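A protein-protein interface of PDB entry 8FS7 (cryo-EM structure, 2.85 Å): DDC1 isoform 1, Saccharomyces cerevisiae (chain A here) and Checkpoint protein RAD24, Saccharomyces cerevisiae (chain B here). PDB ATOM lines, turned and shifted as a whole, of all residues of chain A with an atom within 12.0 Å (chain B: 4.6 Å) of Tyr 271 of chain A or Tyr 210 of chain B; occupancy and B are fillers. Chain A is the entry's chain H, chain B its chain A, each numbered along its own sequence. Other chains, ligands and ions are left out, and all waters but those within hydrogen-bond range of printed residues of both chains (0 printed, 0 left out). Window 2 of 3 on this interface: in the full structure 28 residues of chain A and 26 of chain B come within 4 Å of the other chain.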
ATOM      1  N   PHE A 266      -3.274  29.248  28.314  1.00  0.00           N
ATOM      2  CA  PHE A 266      -2.359  28.294  27.706  1.00  0.00           C
ATOM      3  C   PHE A 266      -2.960  27.763  26.409  1.00  0.00           C
ATOM      4  O   PHE A 266      -4.039  28.179  25.976  1.00  0.00           O
ATOM      5  CB  PHE A 266      -2.041  27.140  28.671  1.00  0.00           C
ATOM      6  CG  PHE A 266      -3.192  26.192  28.893  1.00  0.00           C
ATOM      7  CD1 PHE A 266      -4.173  26.475  29.826  1.00  0.00           C
ATOM      8  CD2 PHE A 266      -3.300  25.024  28.151  1.00  0.00           C
ATOM      9  CE1 PHE A 266      -5.231  25.606  30.019  1.00  0.00           C
ATOM     10  CE2 PHE A 266      -4.354  24.154  28.345  1.00  0.00           C
ATOM     11  CZ  PHE A 266      -5.320  24.445  29.282  1.00  0.00           C
ATOM     12  N   THR A 267      -2.242  26.827  25.790  1.00  0.00           N
ATOM     13  CA  THR A 267      -2.710  26.151  24.587  1.00  0.00           C
ATOM     14  C   THR A 267      -2.072  24.771  24.543  1.00  0.00           C
ATOM     15  O   THR A 267      -0.851  24.650  24.679  1.00  0.00           O
ATOM     16  CB  THR A 267      -2.357  26.956  23.328  1.00  0.00           C
ATOM     17  OG1 THR A 267      -3.307  28.016  23.158  1.00  0.00           O
ATOM     18  CG2 THR A 267      -2.375  26.067  22.095  1.00  0.00           C
ATOM     19  N   LYS A 268      -2.893  23.739  24.367  1.00  0.00           N
ATOM     20  CA  LYS A 268      -2.388  22.375  24.330  1.00  0.00           C
ATOM     21  C   LYS A 268      -1.639  22.108  23.030  1.00  0.00           C
ATOM     22  O   LYS A 268      -1.874  22.755  22.005  1.00  0.00           O
ATOM     23  CB  LYS A 268      -3.530  21.372  24.491  1.00  0.00           C
ATOM     24  CG  LYS A 268      -4.270  21.484  25.814  1.00  0.00           C
ATOM     25  CD  LYS A 268      -5.067  20.225  26.112  1.00  0.00           C
ATOM     26  CE  LYS A 268      -4.154  19.018  26.251  1.00  0.00           C
ATOM     27  NZ  LYS A 268      -4.916  17.768  26.521  1.00  0.00           N
ATOM     28  N   ALA A 269      -0.727  21.141  23.083  1.00  0.00           N
ATOM     29  CA  ALA A 269       0.110  20.785  21.947  1.00  0.00           C
ATOM     30  C   ALA A 269      -0.424  19.532  21.266  1.00  0.00           C
ATOM     31  O   ALA A 269      -0.956  18.632  21.922  1.00  0.00           O
ATOM     32  CB  ALA A 269       1.558  20.560  22.385  1.00  0.00           C
ATOM     33  N   VAL A 270      -0.279  19.482  19.944  1.00  0.00           N
ATOM     34  CA  VAL A 270      -0.720  18.354  19.134  1.00  0.00           C
ATOM     35  C   VAL A 270       0.499  17.725  18.473  1.00  0.00           C
ATOM     36  O   VAL A 270       1.336  18.429  17.896  1.00  0.00           O
ATOM     37  CB  VAL A 270      -1.757  18.783  18.077  1.00  0.00           C
ATOM     38  CG1 VAL A 270      -2.392  17.562  17.430  1.00  0.00           C
ATOM     39  CG2 VAL A 270      -2.819  19.672  18.705  1.00  0.00           C
ATOM     40  N   TYR A 271       0.596  16.402  18.558  1.00  0.00           N
ATOM     41  CA  TYR A 271       1.727  15.656  18.027  1.00  0.00           C
ATOM     42  C   TYR A 271       1.354  15.015  16.697  1.00  0.00           C
ATOM     43  O   TYR A 271       0.224  14.552  16.514  1.00  0.00           O
ATOM     44  CB  TYR A 271       2.188  14.582  19.017  1.00  0.00           C
ATOM     45  CG  TYR A 271       2.678  15.143  20.332  1.00  0.00           C
ATOM     46  CD1 TYR A 271       3.934  15.725  20.436  1.00  0.00           C
ATOM     47  CD2 TYR A 271       1.882  15.095  21.470  1.00  0.00           C
ATOM     48  CE1 TYR A 271       4.387  16.240  21.636  1.00  0.00           C
ATOM     49  CE2 TYR A 271       2.326  15.608  22.674  1.00  0.00           C
ATOM     50  CZ  TYR A 271       3.579  16.179  22.751  1.00  0.00           C
ATOM     51  OH  TYR A 271       4.025  16.691  23.948  1.00  0.00           O
ATOM     52  N   GLY A 272       2.313  14.986  15.775  1.00  0.00           N
ATOM     53  CA  GLY A 272       2.086  14.467  14.443  1.00  0.00           C
ATOM     54  C   GLY A 272       2.224  12.959  14.370  1.00  0.00           C
ATOM     55  O   GLY A 272       2.101  12.241  15.365  1.00  0.00           O
ATOM     56  N   LYS A 273       2.476  12.476  13.151  1.00  0.00           N
ATOM     57  CA  LYS A 273       2.601  11.047  12.890  1.00  0.00           C
ATOM     58  C   LYS A 273       3.780  10.439  13.640  1.00  0.00           C
ATOM     59  O   LYS A 273       3.593   9.585  14.514  1.00  0.00           O
ATOM     60  CB  LYS A 273       2.750  10.792  11.389  1.00  0.00           C
ATOM     61  CG  LYS A 273       2.763   9.320  11.007  1.00  0.00           C
ATOM     62  CD  LYS A 273       2.803   9.138   9.498  1.00  0.00           C
ATOM     63  CE  LYS A 273       1.654   9.864   8.818  1.00  0.00           C
ATOM     64  NZ  LYS A 273       1.703   9.714   7.337  1.00  0.00           N
ATOM     65  N   ASN A 274       4.995  10.870  13.308  1.00  0.00           N
ATOM     66  CA  ASN A 274       6.202  10.359  13.959  1.00  0.00           C
ATOM     67  C   ASN A 274       6.630  11.287  15.097  1.00  0.00           C
ATOM     68  O   ASN A 274       7.756  11.784  15.150  1.00  0.00           O
ATOM     69  CB  ASN A 274       7.317  10.182  12.935  1.00  0.00           C
ATOM     70  CG  ASN A 274       6.946   9.209  11.832  1.00  0.00           C
ATOM     71  OD1 ASN A 274       5.997   8.437  11.964  1.00  0.00           O
ATOM     72  ND2 ASN A 274       7.697   9.242  10.737  1.00  0.00           N
ATOM     73  N   ASN A 275       5.691  11.501  16.023  1.00  0.00           N
ATOM     74  CA  ASN A 275       5.895  12.354  17.197  1.00  0.00           C
ATOM     75  C   ASN A 275       6.358  13.753  16.795  1.00  0.00           C
ATOM     76  O   ASN A 275       7.273  14.327  17.389  1.00  0.00           O
ATOM     77  CB  ASN A 275       6.874  11.711  18.182  1.00  0.00           C
ATOM     78  CG  ASN A 275       6.747  12.276  19.584  1.00  0.00           C
ATOM     79  OD1 ASN A 275       5.643  12.406  20.115  1.00  0.00           O
ATOM     80  ND2 ASN A 275       7.878  12.614  20.192  1.00  0.00           N
ATOM     81  N   ASP A 276       5.720  14.307  15.767  1.00  0.00           N
ATOM     82  CA  ASP A 276       6.030  15.651  15.300  1.00  0.00           C
ATOM     83  C   ASP A 276       5.313  16.669  16.185  1.00  0.00           C
ATOM     84  O   ASP A 276       4.783  16.341  17.250  1.00  0.00           O
ATOM     85  CB  ASP A 276       5.650  15.800  13.828  1.00  0.00           C
ATOM     86  CG  ASP A 276       6.270  14.726  12.955  1.00  0.00           C
ATOM     87  OD1 ASP A 276       7.411  14.923  12.488  1.00  0.00           O
ATOM     88  OD2 ASP A 276       5.616  13.686  12.735  1.00  0.00           O
ATOM     89  N   LEU A 277       5.299  17.930  15.760  1.00  0.00           N
ATOM     90  CA  LEU A 277       4.575  18.993  16.456  1.00  0.00           C
ATOM     91  C   LEU A 277       3.641  19.674  15.463  1.00  0.00           C
ATOM     92  O   LEU A 277       4.071  20.496  14.649  1.00  0.00           O
ATOM     93  CB  LEU A 277       5.528  20.000  17.098  1.00  0.00           C
ATOM     94  CG  LEU A 277       5.253  20.282  18.578  1.00  0.00           C
ATOM     95  CD1 LEU A 277       5.105  18.987  19.365  1.00  0.00           C
ATOM     96  CD2 LEU A 277       6.323  21.174  19.183  1.00  0.00           C
ATOM     97  N   LEU A 278       2.356  19.325  15.531  1.00  0.00           N
ATOM     98  CA  LEU A 278       1.360  20.030  14.733  1.00  0.00           C
ATOM     99  C   LEU A 278       1.052  21.403  15.316  1.00  0.00           C
ATOM    100  O   LEU A 278       0.686  22.322  14.573  1.00  0.00           O
ATOM    101  CB  LEU A 278       0.084  19.196  14.629  1.00  0.00           C
ATOM    102  CG  LEU A 278       0.221  17.824  13.963  1.00  0.00           C
ATOM    103  CD1 LEU A 278      -1.134  17.148  13.838  1.00  0.00           C
ATOM    104  CD2 LEU A 278       0.887  17.952  12.601  1.00  0.00           C
ATOM    105  N   ARG A 279       1.193  21.562  16.630  1.00  0.00           N
ATOM    106  CA  ARG A 279       0.905  22.824  17.295  1.00  0.00           C
ATOM    107  C   ARG A 279       1.758  22.924  18.552  1.00  0.00           C
ATOM    108  O   ARG A 279       1.962  21.929  19.252  1.00  0.00           O
ATOM    109  CB  ARG A 279      -0.584  22.937  17.641  1.00  0.00           C
ATOM    110  CG  ARG A 279      -1.006  24.284  18.199  1.00  0.00           C
ATOM    111  CD  ARG A 279      -2.518  24.441  18.152  1.00  0.00           C
ATOM    112  NE  ARG A 279      -2.966  25.649  18.831  1.00  0.00           N
ATOM    113  CZ  ARG A 279      -3.020  26.849  18.269  1.00  0.00           C
ATOM    114  NH1 ARG A 279      -2.659  27.040  17.011  1.00  0.00           N
ATOM    115  NH2 ARG A 279      -3.448  27.884  18.988  1.00  0.00           N
ATOM    116  N   ASN A 280       2.252  24.128  18.831  1.00  0.00           N
ATOM    117  CA  ASN A 280       3.095  24.359  19.995  1.00  0.00           C
ATOM    118  C   ASN A 280       2.237  24.502  21.252  1.00  0.00           C
ATOM    119  O   ASN A 280       1.004  24.484  21.205  1.00  0.00           O
ATOM    120  CB  ASN A 280       3.970  25.591  19.780  1.00  0.00           C
ATOM    121  CG  ASN A 280       4.944  25.421  18.631  1.00  0.00           C
ATOM    122  OD1 ASN A 280       4.815  24.500  17.824  1.00  0.00           O
ATOM    123  ND2 ASN A 280       5.928  26.308  18.552  1.00  0.00           N
ATOM    124  N   ALA A 281       2.902  24.649  22.399  1.00  0.00           N
ATOM    125  CA  ALA A 281       2.237  24.746  23.700  1.00  0.00           C
ATOM    126  C   ALA A 281       2.770  25.969  24.442  1.00  0.00           C
ATOM    127  O   ALA A 281       3.704  25.864  25.240  1.00  0.00           O
ATOM    128  CB  ALA A 281       2.438  23.468  24.509  1.00  0.00           C
ATOM    129  N   LEU A 282       2.158  27.124  24.192  1.00  0.00           N
ATOM    130  CA  LEU A 282       2.514  28.358  24.879  1.00  0.00           C
ATOM    131  C   LEU A 282       1.614  28.520  26.098  1.00  0.00           C
ATOM    132  O   LEU A 282       0.386  28.438  25.984  1.00  0.00           O
ATOM    133  CB  LEU A 282       2.371  29.557  23.938  1.00  0.00           C
ATOM    134  CG  LEU A 282       3.287  30.782  24.079  1.00  0.00           C
ATOM    135  CD1 LEU A 282       2.898  31.839  23.056  1.00  0.00           C
ATOM    136  CD2 LEU A 282       3.273  31.382  25.480  1.00  0.00           C
ATOM    137  N   LEU B 206      -6.425  17.777  10.830  1.00  0.00           N
ATOM    138  CA  LEU B 206      -5.349  16.869  11.212  1.00  0.00           C
ATOM    139  C   LEU B 206      -5.104  16.908  12.715  1.00  0.00           C
ATOM    140  O   LEU B 206      -4.847  15.870  13.335  1.00  0.00           O
ATOM    141  CB  LEU B 206      -4.070  17.217  10.452  1.00  0.00           C
ATOM    142  CG  LEU B 206      -3.727  16.328   9.256  1.00  0.00           C
ATOM    143  CD1 LEU B 206      -2.391  16.729   8.652  1.00  0.00           C
ATOM    144  CD2 LEU B 206      -3.716  14.863   9.664  1.00  0.00           C
ATOM    145  N   GLN B 207      -5.175  18.098  13.317  1.00  0.00           N
ATOM    146  CA  GLN B 207      -5.006  18.218  14.760  1.00  0.00           C
ATOM    147  C   GLN B 207      -6.145  17.566  15.531  1.00  0.00           C
ATOM    148  O   GLN B 207      -5.924  17.090  16.649  1.00  0.00           O
ATOM    149  CB  GLN B 207      -4.882  19.688  15.161  1.00  0.00           C
ATOM    150  CG  GLN B 207      -3.550  20.323  14.796  1.00  0.00           C
ATOM    151  CD  GLN B 207      -3.637  21.831  14.680  1.00  0.00           C
ATOM    152  OE1 GLN B 207      -4.631  22.440  15.075  1.00  0.00           O
ATOM    153  NE2 GLN B 207      -2.593  22.444  14.133  1.00  0.00           N
ATOM    154  N   TRP B 208      -7.355  17.544  14.968  1.00  0.00           N
ATOM    155  CA  TRP B 208      -8.469  16.867  15.621  1.00  0.00           C
ATOM    156  C   TRP B 208      -8.236  15.362  15.701  1.00  0.00           C
ATOM    157  O   TRP B 208      -8.503  14.745  16.739  1.00  0.00           O
ATOM    158  CB  TRP B 208      -9.773  17.169  14.878  1.00  0.00           C
ATOM    159  CG  TRP B 208     -11.003  16.590  15.520  1.00  0.00           C
ATOM    160  CD1 TRP B 208     -11.429  15.294  15.462  1.00  0.00           C
ATOM    161  CD2 TRP B 208     -11.971  17.293  16.309  1.00  0.00           C
ATOM    162  NE1 TRP B 208     -12.596  15.146  16.169  1.00  0.00           N
ATOM    163  CE2 TRP B 208     -12.951  16.358  16.698  1.00  0.00           C
ATOM    164  CE3 TRP B 208     -12.103  18.621  16.726  1.00  0.00           C
ATOM    165  CZ2 TRP B 208     -14.047  16.708  17.483  1.00  0.00           C
ATOM    166  CZ3 TRP B 208     -13.193  18.967  17.505  1.00  0.00           C
ATOM    167  CH2 TRP B 208     -14.150  18.014  17.875  1.00  0.00           C
ATOM    168  N   LEU B 209      -7.738  14.759  14.619  1.00  0.00           N
ATOM    169  CA  LEU B 209      -7.465  13.325  14.625  1.00  0.00           C
ATOM    170  C   LEU B 209      -6.303  12.985  15.550  1.00  0.00           C
ATOM    171  O   LEU B 209      -6.322  11.950  16.226  1.00  0.00           O
ATOM    172  CB  LEU B 209      -7.177  12.840  13.204  1.00  0.00           C
ATOM    173  CG  LEU B 209      -8.315  12.967  12.190  1.00  0.00           C
ATOM    174  CD1 LEU B 209      -7.816  12.673  10.786  1.00  0.00           C
ATOM    175  CD2 LEU B 209      -9.460  12.039  12.558  1.00  0.00           C
ATOM    176  N   TYR B 210      -5.287  13.841  15.592  1.00  0.00           N
ATOM    177  CA  TYR B 210      -4.105  13.624  16.415  1.00  0.00           C
ATOM    178  C   TYR B 210      -4.205  14.287  17.782  1.00  0.00           C
ATOM    179  O   TYR B 210      -3.195  14.378  18.488  1.00  0.00           O
ATOM    180  CB  TYR B 210      -2.858  14.130  15.685  1.00  0.00           C
ATOM    181  CG  TYR B 210      -2.378  13.219  14.579  1.00  0.00           C
ATOM    182  CD1 TYR B 210      -1.892  11.949  14.860  1.00  0.00           C
ATOM    183  CD2 TYR B 210      -2.406  13.631  13.253  1.00  0.00           C
ATOM    184  CE1 TYR B 210      -1.449  11.114  13.851  1.00  0.00           C
ATOM    185  CE2 TYR B 210      -1.966  12.802  12.238  1.00  0.00           C
ATOM    186  CZ  TYR B 210      -1.489  11.546  12.543  1.00  0.00           C
ATOM    187  OH  TYR B 210      -1.050  10.717  11.536  1.00  0.00           O
ATOM    188  N   SER B 211      -5.390  14.759  18.163  1.00  0.00           N
ATOM    189  CA  SER B 211      -5.551  15.439  19.442  1.00  0.00           C
ATOM    190  C   SER B 211      -5.328  14.477  20.601  1.00  0.00           C
ATOM    191  O   SER B 211      -5.708  13.304  20.544  1.00  0.00           O
ATOM    192  CB  SER B 211      -6.945  16.059  19.539  1.00  0.00           C
ATOM    193  OG  SER B 211      -7.135  16.693  20.791  1.00  0.00           O
ATOM    194  N   SER B 212      -4.706  14.987  21.661  1.00  0.00           N
ATOM    195  CA  SER B 212      -4.493  14.233  22.888  1.00  0.00           C
ATOM    196  C   SER B 212      -5.673  14.336  23.845  1.00  0.00           C
ATOM    197  O   SER B 212      -5.544  13.953  25.013  1.00  0.00           O
ATOM    198  CB  SER B 212      -3.215  14.710  23.584  1.00  0.00           C
ATOM    199  OG  SER B 212      -3.241  16.111  23.789  1.00  0.00           O
ATOM    200  N   GLU B 253      -2.584  12.076   4.312  1.00  0.00           N
ATOM    201  CA  GLU B 253      -2.518  11.813   5.747  1.00  0.00           C
ATOM    202  C   GLU B 253      -3.908  11.695   6.361  1.00  0.00           C
ATOM    203  O   GLU B 253      -4.158  10.800   7.179  1.00  0.00           O
ATOM    204  CB  GLU B 253      -1.719  12.914   6.444  1.00  0.00           C
ATOM    205  CG  GLU B 253      -0.689  12.400   7.435  1.00  0.00           C
ATOM    206  CD  GLU B 253       0.108  13.517   8.082  1.00  0.00           C
ATOM    207  OE1 GLU B 253       0.371  14.530   7.403  1.00  0.00           O
ATOM    208  OE2 GLU B 253       0.469  13.379   9.270  1.00  0.00           O
ATOM    209  N   HIS B 257      -5.979   7.482   7.572  1.00  0.00           N
ATOM    210  CA  HIS B 257      -5.774   7.627   9.001  1.00  0.00           C
ATOM    211  C   HIS B 257      -6.529   6.541   9.758  1.00  0.00           C
ATOM    212  O   HIS B 257      -7.666   6.214   9.400  1.00  0.00           O
ATOM    213  CB  HIS B 257      -6.239   9.010   9.484  1.00  0.00           C
ATOM    214  CG  HIS B 257      -5.642   9.425  10.793  1.00  0.00           C
ATOM    215  ND1 HIS B 257      -6.133   8.995  12.006  1.00  0.00           N
ATOM    216  CD2 HIS B 257      -4.594  10.234  11.078  1.00  0.00           C
ATOM    217  CE1 HIS B 257      -5.414   9.520  12.982  1.00  0.00           C
ATOM    218  NE2 HIS B 257      -4.473  10.275  12.446  1.00  0.00           N
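The side-chain amide nitrogen of Gln 207 of chain B lies within hydrogen-bond range of the backbone carbonyl oxygen of Leu 278 of chain A, at 3.3 Å.
Lys 268 of chain A touches Ser 212 of chain B (NZ to OG, 3.6 Å). Ala 269 of chain A touches Ser 212 of chain B. O of Gln 207 of chain B touches CG1 of Val 270 of chain A, 3.6 Å away. Val 270 of chain A touches Tyr 210 of chain B (CG1 to O, 3.4 Å). Tyr 271 of chain A touches Tyr 210 of chain B (O to CB, 3.2 Å). CB of Lys 273 of chain A touches OH of Tyr 210 of chain B, 3.8 Å away. Glu 253 of chain B touches Lys 273 of chain A. CD1 of Leu 278 of chain A touches O of Leu 206 of chain B (3.96 Å). Leu 278 of chain A touches Tyr 210 of chain B.
Printed residues of chain A that touch a printed residue of chain B: Lys 268, Ala 269, Val 270, Tyr 271, Lys 273 and Leu 278. Of the 9 printed residues of chain B, 5 touch a printed residue of chain A. Hydrophobic or aromatic side chains of chain B that line the printed part of chain A: Tyr 210. Among the printed residues, 10 pairs touch across the chains.
The backbone carbonyl oxygen (O) of Val 270 of chain A is in hydrogen-bond range of the backbone NH (N) of Leu 278 of chain A. N of Arg 279 of chain A lies within hydrogen-bond range of O of Val 270 of chain A (3.4 Å). The backbone NH of Lys 273 of chain A sits at hydrogen-bond distance from the side-chain carboxylate of Asp 276 of chain A, at 3.4 Å.
Printed residues of chain B within 4 Å of Lys 268 of chain A: Ser 212. Of the printed residues of chain B, Ala 269 of chain A touches Ser 212 (3.9 Å). Of chain B, only Tyr 210 comes within 4 Å of Tyr 271 of chain A. Of the printed residues of chain B, Lys 273 of chain A touches Tyr 210 (3.8 Å) and Glu 253 (3.6 Å). Asp 276 of chain A touches none of the printed residues of chain B. Of the printed residues of chain B, Leu 278 of chain A touches Leu 206, Gln 207 and Tyr 210. Of the printed residues of chain A, Gln 207 of chain B touches Val 270 (3.6 Å) and Leu 278 (3.3 Å). Leu 209 of chain B touches none of the printed residues of chain A. Of chain A, only Val 270, Tyr 271, Lys 273 and Leu 278 come within 4 Å of Tyr 210 of chain B. Ser 212 of chain B touches just these residues of chain A: Lys 268 (3.6 Å) and Ala 269 (3.9 Å). Of chain A, only Lys 273 comes within 4 Å of Glu 253 of chain B. The nearest printed residue of chain B that does not touch Tyr 271 of chain A is Ser 212 of chain B (5.5 Å). The nearest residue of chain A that does not touch Tyr 210 of chain B is Gly 272 of chain A (4.02 Å).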
